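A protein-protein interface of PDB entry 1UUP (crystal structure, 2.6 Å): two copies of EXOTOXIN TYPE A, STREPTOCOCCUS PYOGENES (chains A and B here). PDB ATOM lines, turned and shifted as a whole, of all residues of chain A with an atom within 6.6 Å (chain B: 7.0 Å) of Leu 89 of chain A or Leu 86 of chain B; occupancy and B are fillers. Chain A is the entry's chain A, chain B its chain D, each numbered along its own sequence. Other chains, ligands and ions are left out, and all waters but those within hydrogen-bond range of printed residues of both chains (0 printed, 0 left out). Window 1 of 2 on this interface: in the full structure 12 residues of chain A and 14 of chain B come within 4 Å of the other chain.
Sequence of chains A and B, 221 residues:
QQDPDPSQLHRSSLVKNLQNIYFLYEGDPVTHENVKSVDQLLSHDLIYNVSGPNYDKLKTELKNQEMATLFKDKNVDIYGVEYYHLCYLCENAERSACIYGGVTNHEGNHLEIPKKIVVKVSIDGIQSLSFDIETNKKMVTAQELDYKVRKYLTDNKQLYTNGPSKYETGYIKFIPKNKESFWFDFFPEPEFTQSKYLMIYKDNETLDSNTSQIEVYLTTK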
ATOM      1  N   LEU A  41      -9.535  -4.905  38.413  1.00  0.00           N
ATOM      2  CA  LEU A  41      -9.006  -6.198  38.821  1.00  0.00           C
ATOM      3  C   LEU A  41      -9.074  -6.318  40.343  1.00  0.00           C
ATOM      4  O   LEU A  41      -9.848  -7.116  40.873  1.00  0.00           O
ATOM      5  CB  LEU A  41      -7.567  -6.358  38.328  1.00  0.00           C
ATOM      6  CG  LEU A  41      -6.918  -7.720  38.595  1.00  0.00           C
ATOM      7  CD1 LEU A  41      -7.894  -8.826  38.247  1.00  0.00           C
ATOM      8  CD2 LEU A  41      -5.631  -7.847  37.783  1.00  0.00           C
ATOM      9  N   TYR A  84       5.016  -2.944  30.756  1.00  0.00           N
ATOM     10  CA  TYR A  84       4.265  -4.117  30.306  1.00  0.00           C
ATOM     11  C   TYR A  84       4.693  -5.429  30.957  1.00  0.00           C
ATOM     12  O   TYR A  84       3.869  -6.315  31.186  1.00  0.00           O
ATOM     13  CB  TYR A  84       4.348  -4.252  28.773  1.00  0.00           C
ATOM     14  CG  TYR A  84       3.946  -2.990  28.036  1.00  0.00           C
ATOM     15  CD1 TYR A  84       4.805  -1.884  27.984  1.00  0.00           C
ATOM     16  CD2 TYR A  84       2.687  -2.872  27.444  1.00  0.00           C
ATOM     17  CE1 TYR A  84       4.412  -0.685  27.365  1.00  0.00           C
ATOM     18  CE2 TYR A  84       2.286  -1.676  26.821  1.00  0.00           C
ATOM     19  CZ  TYR A  84       3.151  -0.586  26.787  1.00  0.00           C
ATOM     20  OH  TYR A  84       2.760   0.602  26.189  1.00  0.00           O
ATOM     21  N   LEU A  86       5.039  -8.196  33.279  1.00  0.00           N
ATOM     22  CA  LEU A  86       4.332  -8.573  34.499  1.00  0.00           C
ATOM     23  C   LEU A  86       3.268  -7.510  34.747  1.00  0.00           C
ATOM     24  O   LEU A  86       3.189  -6.944  35.838  1.00  0.00           O
ATOM     25  CB  LEU A  86       5.293  -8.593  35.695  1.00  0.00           C
ATOM     26  CG  LEU A  86       6.673  -9.250  35.562  1.00  0.00           C
ATOM     27  CD1 LEU A  86       7.526  -8.876  36.778  1.00  0.00           C
ATOM     28  CD2 LEU A  86       6.528 -10.766  35.425  1.00  0.00           C
ATOM     29  N   CYS A  87       2.455  -7.228  33.738  1.00  0.00           N
ATOM     30  CA  CYS A  87       1.431  -6.210  33.883  1.00  0.00           C
ATOM     31  C   CYS A  87       0.079  -6.795  34.256  1.00  0.00           C
ATOM     32  O   CYS A  87      -0.319  -6.781  35.423  1.00  0.00           O
ATOM     33  CB  CYS A  87       1.340  -5.390  32.583  1.00  0.00           C
ATOM     34  SG  CYS A  87      -0.070  -4.238  32.366  1.00  0.00           S
ATOM     35  N   TYR A  88      -0.618  -7.324  33.265  1.00  0.00           N
ATOM     36  CA  TYR A  88      -1.941  -7.874  33.478  1.00  0.00           C
ATOM     37  C   TYR A  88      -1.898  -9.309  32.982  1.00  0.00           C
ATOM     38  O   TYR A  88      -1.994  -9.567  31.782  1.00  0.00           O
ATOM     39  CB  TYR A  88      -2.940  -7.033  32.673  1.00  0.00           C
ATOM     40  CG  TYR A  88      -4.410  -7.322  32.881  1.00  0.00           C
ATOM     41  CD1 TYR A  88      -4.918  -8.614  32.754  1.00  0.00           C
ATOM     42  CD2 TYR A  88      -5.309  -6.280  33.128  1.00  0.00           C
ATOM     43  CE1 TYR A  88      -6.280  -8.864  32.862  1.00  0.00           C
ATOM     44  CE2 TYR A  88      -6.675  -6.515  33.237  1.00  0.00           C
ATOM     45  CZ  TYR A  88      -7.154  -7.812  33.102  1.00  0.00           C
ATOM     46  OH  TYR A  88      -8.509  -8.056  33.198  1.00  0.00           O
ATOM     47  N   LEU A  89      -1.740 -10.244  33.911  1.00  0.00           N
ATOM     48  CA  LEU A  89      -1.670 -11.660  33.560  1.00  0.00           C
ATOM     49  C   LEU A  89      -2.993 -12.375  33.835  1.00  0.00           C
ATOM     50  O   LEU A  89      -3.216 -12.862  34.945  1.00  0.00           O
ATOM     51  CB  LEU A  89      -0.545 -12.316  34.357  1.00  0.00           C
ATOM     52  CG  LEU A  89       0.838 -11.702  34.130  1.00  0.00           C
ATOM     53  CD1 LEU A  89       1.790 -12.158  35.221  1.00  0.00           C
ATOM     54  CD2 LEU A  89       1.348 -12.087  32.742  1.00  0.00           C
ATOM     55  N   CYS A  90      -3.862 -12.447  32.825  1.00  0.00           N
ATOM     56  CA  CYS A  90      -5.165 -13.091  32.993  1.00  0.00           C
ATOM     57  C   CYS A  90      -5.760 -13.701  31.725  1.00  0.00           C
ATOM     58  O   CYS A  90      -6.973 -13.914  31.645  1.00  0.00           O
ATOM     59  CB  CYS A  90      -6.153 -12.090  33.600  1.00  0.00           C
ATOM     60  SG  CYS A  90      -5.687 -11.667  35.301  1.00  0.00           S
ATOM     61  N   GLU A  91      -4.905 -13.989  30.747  1.00  0.00           N
ATOM     62  CA  GLU A  91      -5.331 -14.583  29.481  1.00  0.00           C
ATOM     63  C   GLU A  91      -6.744 -14.228  28.994  1.00  0.00           C
ATOM     64  O   GLU A  91      -7.418 -15.057  28.372  1.00  0.00           O
ATOM     65  CB  GLU A  91      -5.179 -16.110  29.543  1.00  0.00           C
ATOM     66  CG  GLU A  91      -5.595 -16.743  30.861  1.00  0.00           C
ATOM     67  CD  GLU A  91      -4.440 -16.868  31.841  1.00  0.00           C
ATOM     68  OE1 GLU A  91      -3.528 -17.687  31.589  1.00  0.00           O
ATOM     69  OE2 GLU A  91      -4.442 -16.147  32.862  1.00  0.00           O
ATOM     70  N   ASN A  92      -7.188 -13.004  29.275  1.00  0.00           N
ATOM     71  CA  ASN A  92      -8.507 -12.532  28.841  1.00  0.00           C
ATOM     72  C   ASN A  92      -8.355 -11.063  28.478  1.00  0.00           C
ATOM     73  O   ASN A  92      -9.330 -10.345  28.241  1.00  0.00           O
ATOM     74  CB  ASN A  92      -9.552 -12.680  29.949  1.00  0.00           C
ATOM     75  CG  ASN A  92      -9.416 -11.630  31.029  1.00  0.00           C
ATOM     76  OD1 ASN A  92     -10.380 -11.329  31.732  1.00  0.00           O
ATOM     77  ND2 ASN A  92      -8.217 -11.072  31.177  1.00  0.00           N
ATOM     78  N   ALA A  93      -7.099 -10.640  28.473  1.00  0.00           N
ATOM     79  CA  ALA A  93      -6.680  -9.290  28.125  1.00  0.00           C
ATOM     80  C   ALA A  93      -5.206  -9.510  27.815  1.00  0.00           C
ATOM     81  O   ALA A  93      -4.412  -9.801  28.710  1.00  0.00           O
ATOM     82  CB  ALA A  93      -6.850  -8.349  29.302  1.00  0.00           C
ATOM     83  N   GLU A  94      -4.855  -9.412  26.541  1.00  0.00           N
ATOM     84  CA  GLU A  94      -3.485  -9.638  26.120  1.00  0.00           C
ATOM     85  C   GLU A  94      -2.802  -8.392  25.603  1.00  0.00           C
ATOM     86  O   GLU A  94      -1.696  -8.474  25.083  1.00  0.00           O
ATOM     87  CB  GLU A  94      -3.443 -10.695  25.026  1.00  0.00           C
ATOM     88  CG  GLU A  94      -4.385 -11.849  25.242  1.00  0.00           C
ATOM     89  CD  GLU A  94      -3.973 -13.063  24.445  1.00  0.00           C
ATOM     90  OE1 GLU A  94      -4.846 -13.901  24.141  1.00  0.00           O
ATOM     91  OE2 GLU A  94      -2.770 -13.183  24.128  1.00  0.00           O
ATOM     92  N   LYS B  59      12.798 -14.749  22.179  1.00  0.00           N
ATOM     93  CA  LYS B  59      12.812 -16.162  22.525  1.00  0.00           C
ATOM     94  C   LYS B  59      11.916 -16.941  21.567  1.00  0.00           C
ATOM     95  O   LYS B  59      10.705 -16.713  21.513  1.00  0.00           O
ATOM     96  CB  LYS B  59      12.342 -16.383  23.971  1.00  0.00           C
ATOM     97  CG  LYS B  59      12.428 -17.848  24.419  1.00  0.00           C
ATOM     98  CD  LYS B  59      12.097 -18.029  25.898  1.00  0.00           C
ATOM     99  CE  LYS B  59      10.625 -17.745  26.207  1.00  0.00           C
ATOM    100  NZ  LYS B  59       9.702 -18.753  25.604  1.00  0.00           N
ATOM    101  N   TYR B  83       4.625 -12.281  19.919  1.00  0.00           N
ATOM    102  CA  TYR B  83       3.617 -11.885  20.893  1.00  0.00           C
ATOM    103  C   TYR B  83       4.312 -11.487  22.195  1.00  0.00           C
ATOM    104  O   TYR B  83       5.476 -11.822  22.411  1.00  0.00           O
ATOM    105  CB  TYR B  83       2.644 -13.047  21.139  1.00  0.00           C
ATOM    106  CG  TYR B  83       3.275 -14.271  21.767  1.00  0.00           C
ATOM    107  CD1 TYR B  83       3.267 -14.455  23.145  1.00  0.00           C
ATOM    108  CD2 TYR B  83       3.892 -15.237  20.983  1.00  0.00           C
ATOM    109  CE1 TYR B  83       3.853 -15.569  23.732  1.00  0.00           C
ATOM    110  CE2 TYR B  83       4.490 -16.356  21.559  1.00  0.00           C
ATOM    111  CZ  TYR B  83       4.463 -16.517  22.937  1.00  0.00           C
ATOM    112  OH  TYR B  83       5.042 -17.632  23.508  1.00  0.00           O
ATOM    113  N   TYR B  84       3.607 -10.784  23.069  1.00  0.00           N
ATOM    114  CA  TYR B  84       4.222 -10.373  24.320  1.00  0.00           C
ATOM    115  C   TYR B  84       3.490 -10.882  25.547  1.00  0.00           C
ATOM    116  O   TYR B  84       4.115 -11.137  26.579  1.00  0.00           O
ATOM    117  CB  TYR B  84       4.341  -8.844  24.381  1.00  0.00           C
ATOM    118  CG  TYR B  84       5.052  -8.263  23.190  1.00  0.00           C
ATOM    119  CD1 TYR B  84       4.377  -8.077  21.985  1.00  0.00           C
ATOM    120  CD2 TYR B  84       6.412  -7.955  23.239  1.00  0.00           C
ATOM    121  CE1 TYR B  84       5.035  -7.604  20.857  1.00  0.00           C
ATOM    122  CE2 TYR B  84       7.086  -7.480  22.107  1.00  0.00           C
ATOM    123  CZ  TYR B  84       6.385  -7.313  20.918  1.00  0.00           C
ATOM    124  OH  TYR B  84       7.023  -6.891  19.770  1.00  0.00           O
ATOM    125  N   HIS B  85       2.172 -11.033  25.446  1.00  0.00           N
ATOM    126  CA  HIS B  85       1.392 -11.514  26.581  1.00  0.00           C
ATOM    127  C   HIS B  85       1.823 -12.923  26.987  1.00  0.00           C
ATOM    128  O   HIS B  85       1.642 -13.875  26.233  1.00  0.00           O
ATOM    129  CB  HIS B  85      -0.105 -11.508  26.250  1.00  0.00           C
ATOM    130  CG  HIS B  85      -0.978 -11.891  27.406  1.00  0.00           C
ATOM    131  ND1 HIS B  85      -0.867 -11.302  28.648  1.00  0.00           N
ATOM    132  CD2 HIS B  85      -1.994 -12.783  27.504  1.00  0.00           C
ATOM    133  CE1 HIS B  85      -1.776 -11.814  29.459  1.00  0.00           C
ATOM    134  NE2 HIS B  85      -2.474 -12.714  28.790  1.00  0.00           N
ATOM    135  N   LEU B  86       2.397 -13.037  28.181  1.00  0.00           N
ATOM    136  CA  LEU B  86       2.858 -14.319  28.712  1.00  0.00           C
ATOM    137  C   LEU B  86       4.135 -14.757  28.002  1.00  0.00           C
ATOM    138  O   LEU B  86       4.239 -15.874  27.497  1.00  0.00           O
ATOM    139  CB  LEU B  86       1.767 -15.380  28.539  1.00  0.00           C
ATOM    140  CG  LEU B  86       0.376 -14.910  28.971  1.00  0.00           C
ATOM    141  CD1 LEU B  86      -0.625 -16.062  28.836  1.00  0.00           C
ATOM    142  CD2 LEU B  86       0.434 -14.391  30.416  1.00  0.00           C
ATOM    143  N   CYS B  87       5.105 -13.855  27.970  1.00  0.00           N
ATOM    144  CA  CYS B  87       6.383 -14.109  27.329  1.00  0.00           C
ATOM    145  C   CYS B  87       7.491 -13.457  28.131  1.00  0.00           C
ATOM    146  O   CYS B  87       7.461 -12.242  28.368  1.00  0.00           O
ATOM    147  CB  CYS B  87       6.388 -13.521  25.918  1.00  0.00           C
ATOM    148  SG  CYS B  87       8.045 -13.359  25.176  1.00  0.00           S
ATOM    149  N   TYR B  88       8.463 -14.257  28.552  1.00  0.00           N
ATOM    150  CA  TYR B  88       9.595 -13.734  29.308  1.00  0.00           C
ATOM    151  C   TYR B  88      10.484 -14.860  29.795  1.00  0.00           C
ATOM    152  O   TYR B  88      10.053 -16.010  29.897  1.00  0.00           O
ATOM    153  CB  TYR B  88       9.117 -12.886  30.495  1.00  0.00           C
ATOM    154  CG  TYR B  88       8.419 -13.670  31.574  1.00  0.00           C
ATOM    155  CD1 TYR B  88       9.132 -14.223  32.634  1.00  0.00           C
ATOM    156  CD2 TYR B  88       7.042 -13.882  31.525  1.00  0.00           C
ATOM    157  CE1 TYR B  88       8.499 -14.966  33.620  1.00  0.00           C
ATOM    158  CE2 TYR B  88       6.396 -14.626  32.502  1.00  0.00           C
ATOM    159  CZ  TYR B  88       7.131 -15.164  33.546  1.00  0.00           C
ATOM    160  OH  TYR B  88       6.494 -15.906  34.510  1.00  0.00           O
ATOM    161  N   CYS B  98       8.422 -13.065  22.073  1.00  0.00           N
ATOM    162  CA  CYS B  98       8.421 -14.501  21.793  1.00  0.00           C
ATOM    163  C   CYS B  98       7.766 -14.843  20.467  1.00  0.00           C
ATOM    164  O   CYS B  98       6.855 -14.150  19.995  1.00  0.00           O
ATOM    165  CB  CYS B  98       7.687 -15.293  22.890  1.00  0.00           C
ATOM    166  SG  CYS B  98       8.415 -15.267  24.563  1.00  0.00           S
ATOM    167  N   THR B 193      -5.622 -17.727  23.112  1.00  0.00           N
ATOM    168  CA  THR B 193      -4.505 -16.933  23.602  1.00  0.00           C
ATOM    169  C   THR B 193      -3.506 -16.819  22.444  1.00  0.00           C
ATOM    170  O   THR B 193      -3.241 -17.809  21.757  1.00  0.00           O
ATOM    171  CB  THR B 193      -3.858 -17.622  24.837  1.00  0.00           C
ATOM    172  OG1 THR B 193      -3.745 -16.667  25.887  1.00  0.00           O
ATOM    173  CG2 THR B 193      -2.469 -18.194  24.519  1.00  0.00           C
ATOM    174  N   SER B 195      -0.458 -16.824  22.325  1.00  0.00           N
ATOM    175  CA  SER B 195       0.578 -17.827  22.502  1.00  0.00           C
ATOM    176  C   SER B 195       0.148 -19.233  22.078  1.00  0.00           C
ATOM    177  O   SER B 195       0.933 -19.975  21.490  1.00  0.00           O
ATOM    178  CB  SER B 195       1.036 -17.858  23.957  1.00  0.00           C
ATOM    179  OG  SER B 195       2.249 -18.584  24.062  1.00  0.00           O
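Hydrophobic or aromatic side chains of chain A within 4 Å of the printed part of chain B: Leu 89. Among the printed residues, no Asp or Glu carboxylate lies within 4 Å of a Lys or Arg side-chain nitrogen of the other chain.
4 positions are printed for both chains.
Leu 89 of chain A touches one residue of chain B. Of the printed residues of chain A, Leu 86 of chain B touches Leu 89. Of the printed residues of chain A, Thr 193 of chain B touches Glu 91 and Glu 94. Printed residues of chain B within 4 Å of Ala 93 of chain A: His 85 (3.4 Å). Of the printed residues of chain A, His 85 of chain B touches Tyr 88, Glu 91, Ala 93 and Glu 94. Of the printed residues of chain B, Glu 94 of chain A touches His 85 and Thr 193. Of the printed residues of chain B, Tyr 88 of chain A touches His 85. The nearest residue of chain B that does not touch Leu 89 of chain A is His 85 of chain B (4.1 Å). The nearest printed residue of chain B that does not touch Ala 93 of chain A is Leu 86 of chain B (6.9 Å).
The side-chain sulfur of Cys 87 of chain B forms a disulfide with the side-chain sulfur of Cys 98 of chain B (2.0 Å).
OE1 of Glu 94 of chain A sits close to OG1 of Thr 193 of chain B, 3.5 Å away. NE2 of His 85 of chain B lies close to O of Ala 93 of chain A. The backbone NH of Glu 91 of chain A lies within hydrogen-bond range of a ring nitrogen (NE2) of His 85 of chain B (3.4 Å).
O of Tyr 88 of chain A touches CE1 of His 85 of chain B, 3.2 Å away. Leu 89 of chain A touches Leu 86 of chain B. Glu 91 of chain A touches Thr 193 of chain B. Glu 94 of chain A touches His 85 of chain B.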
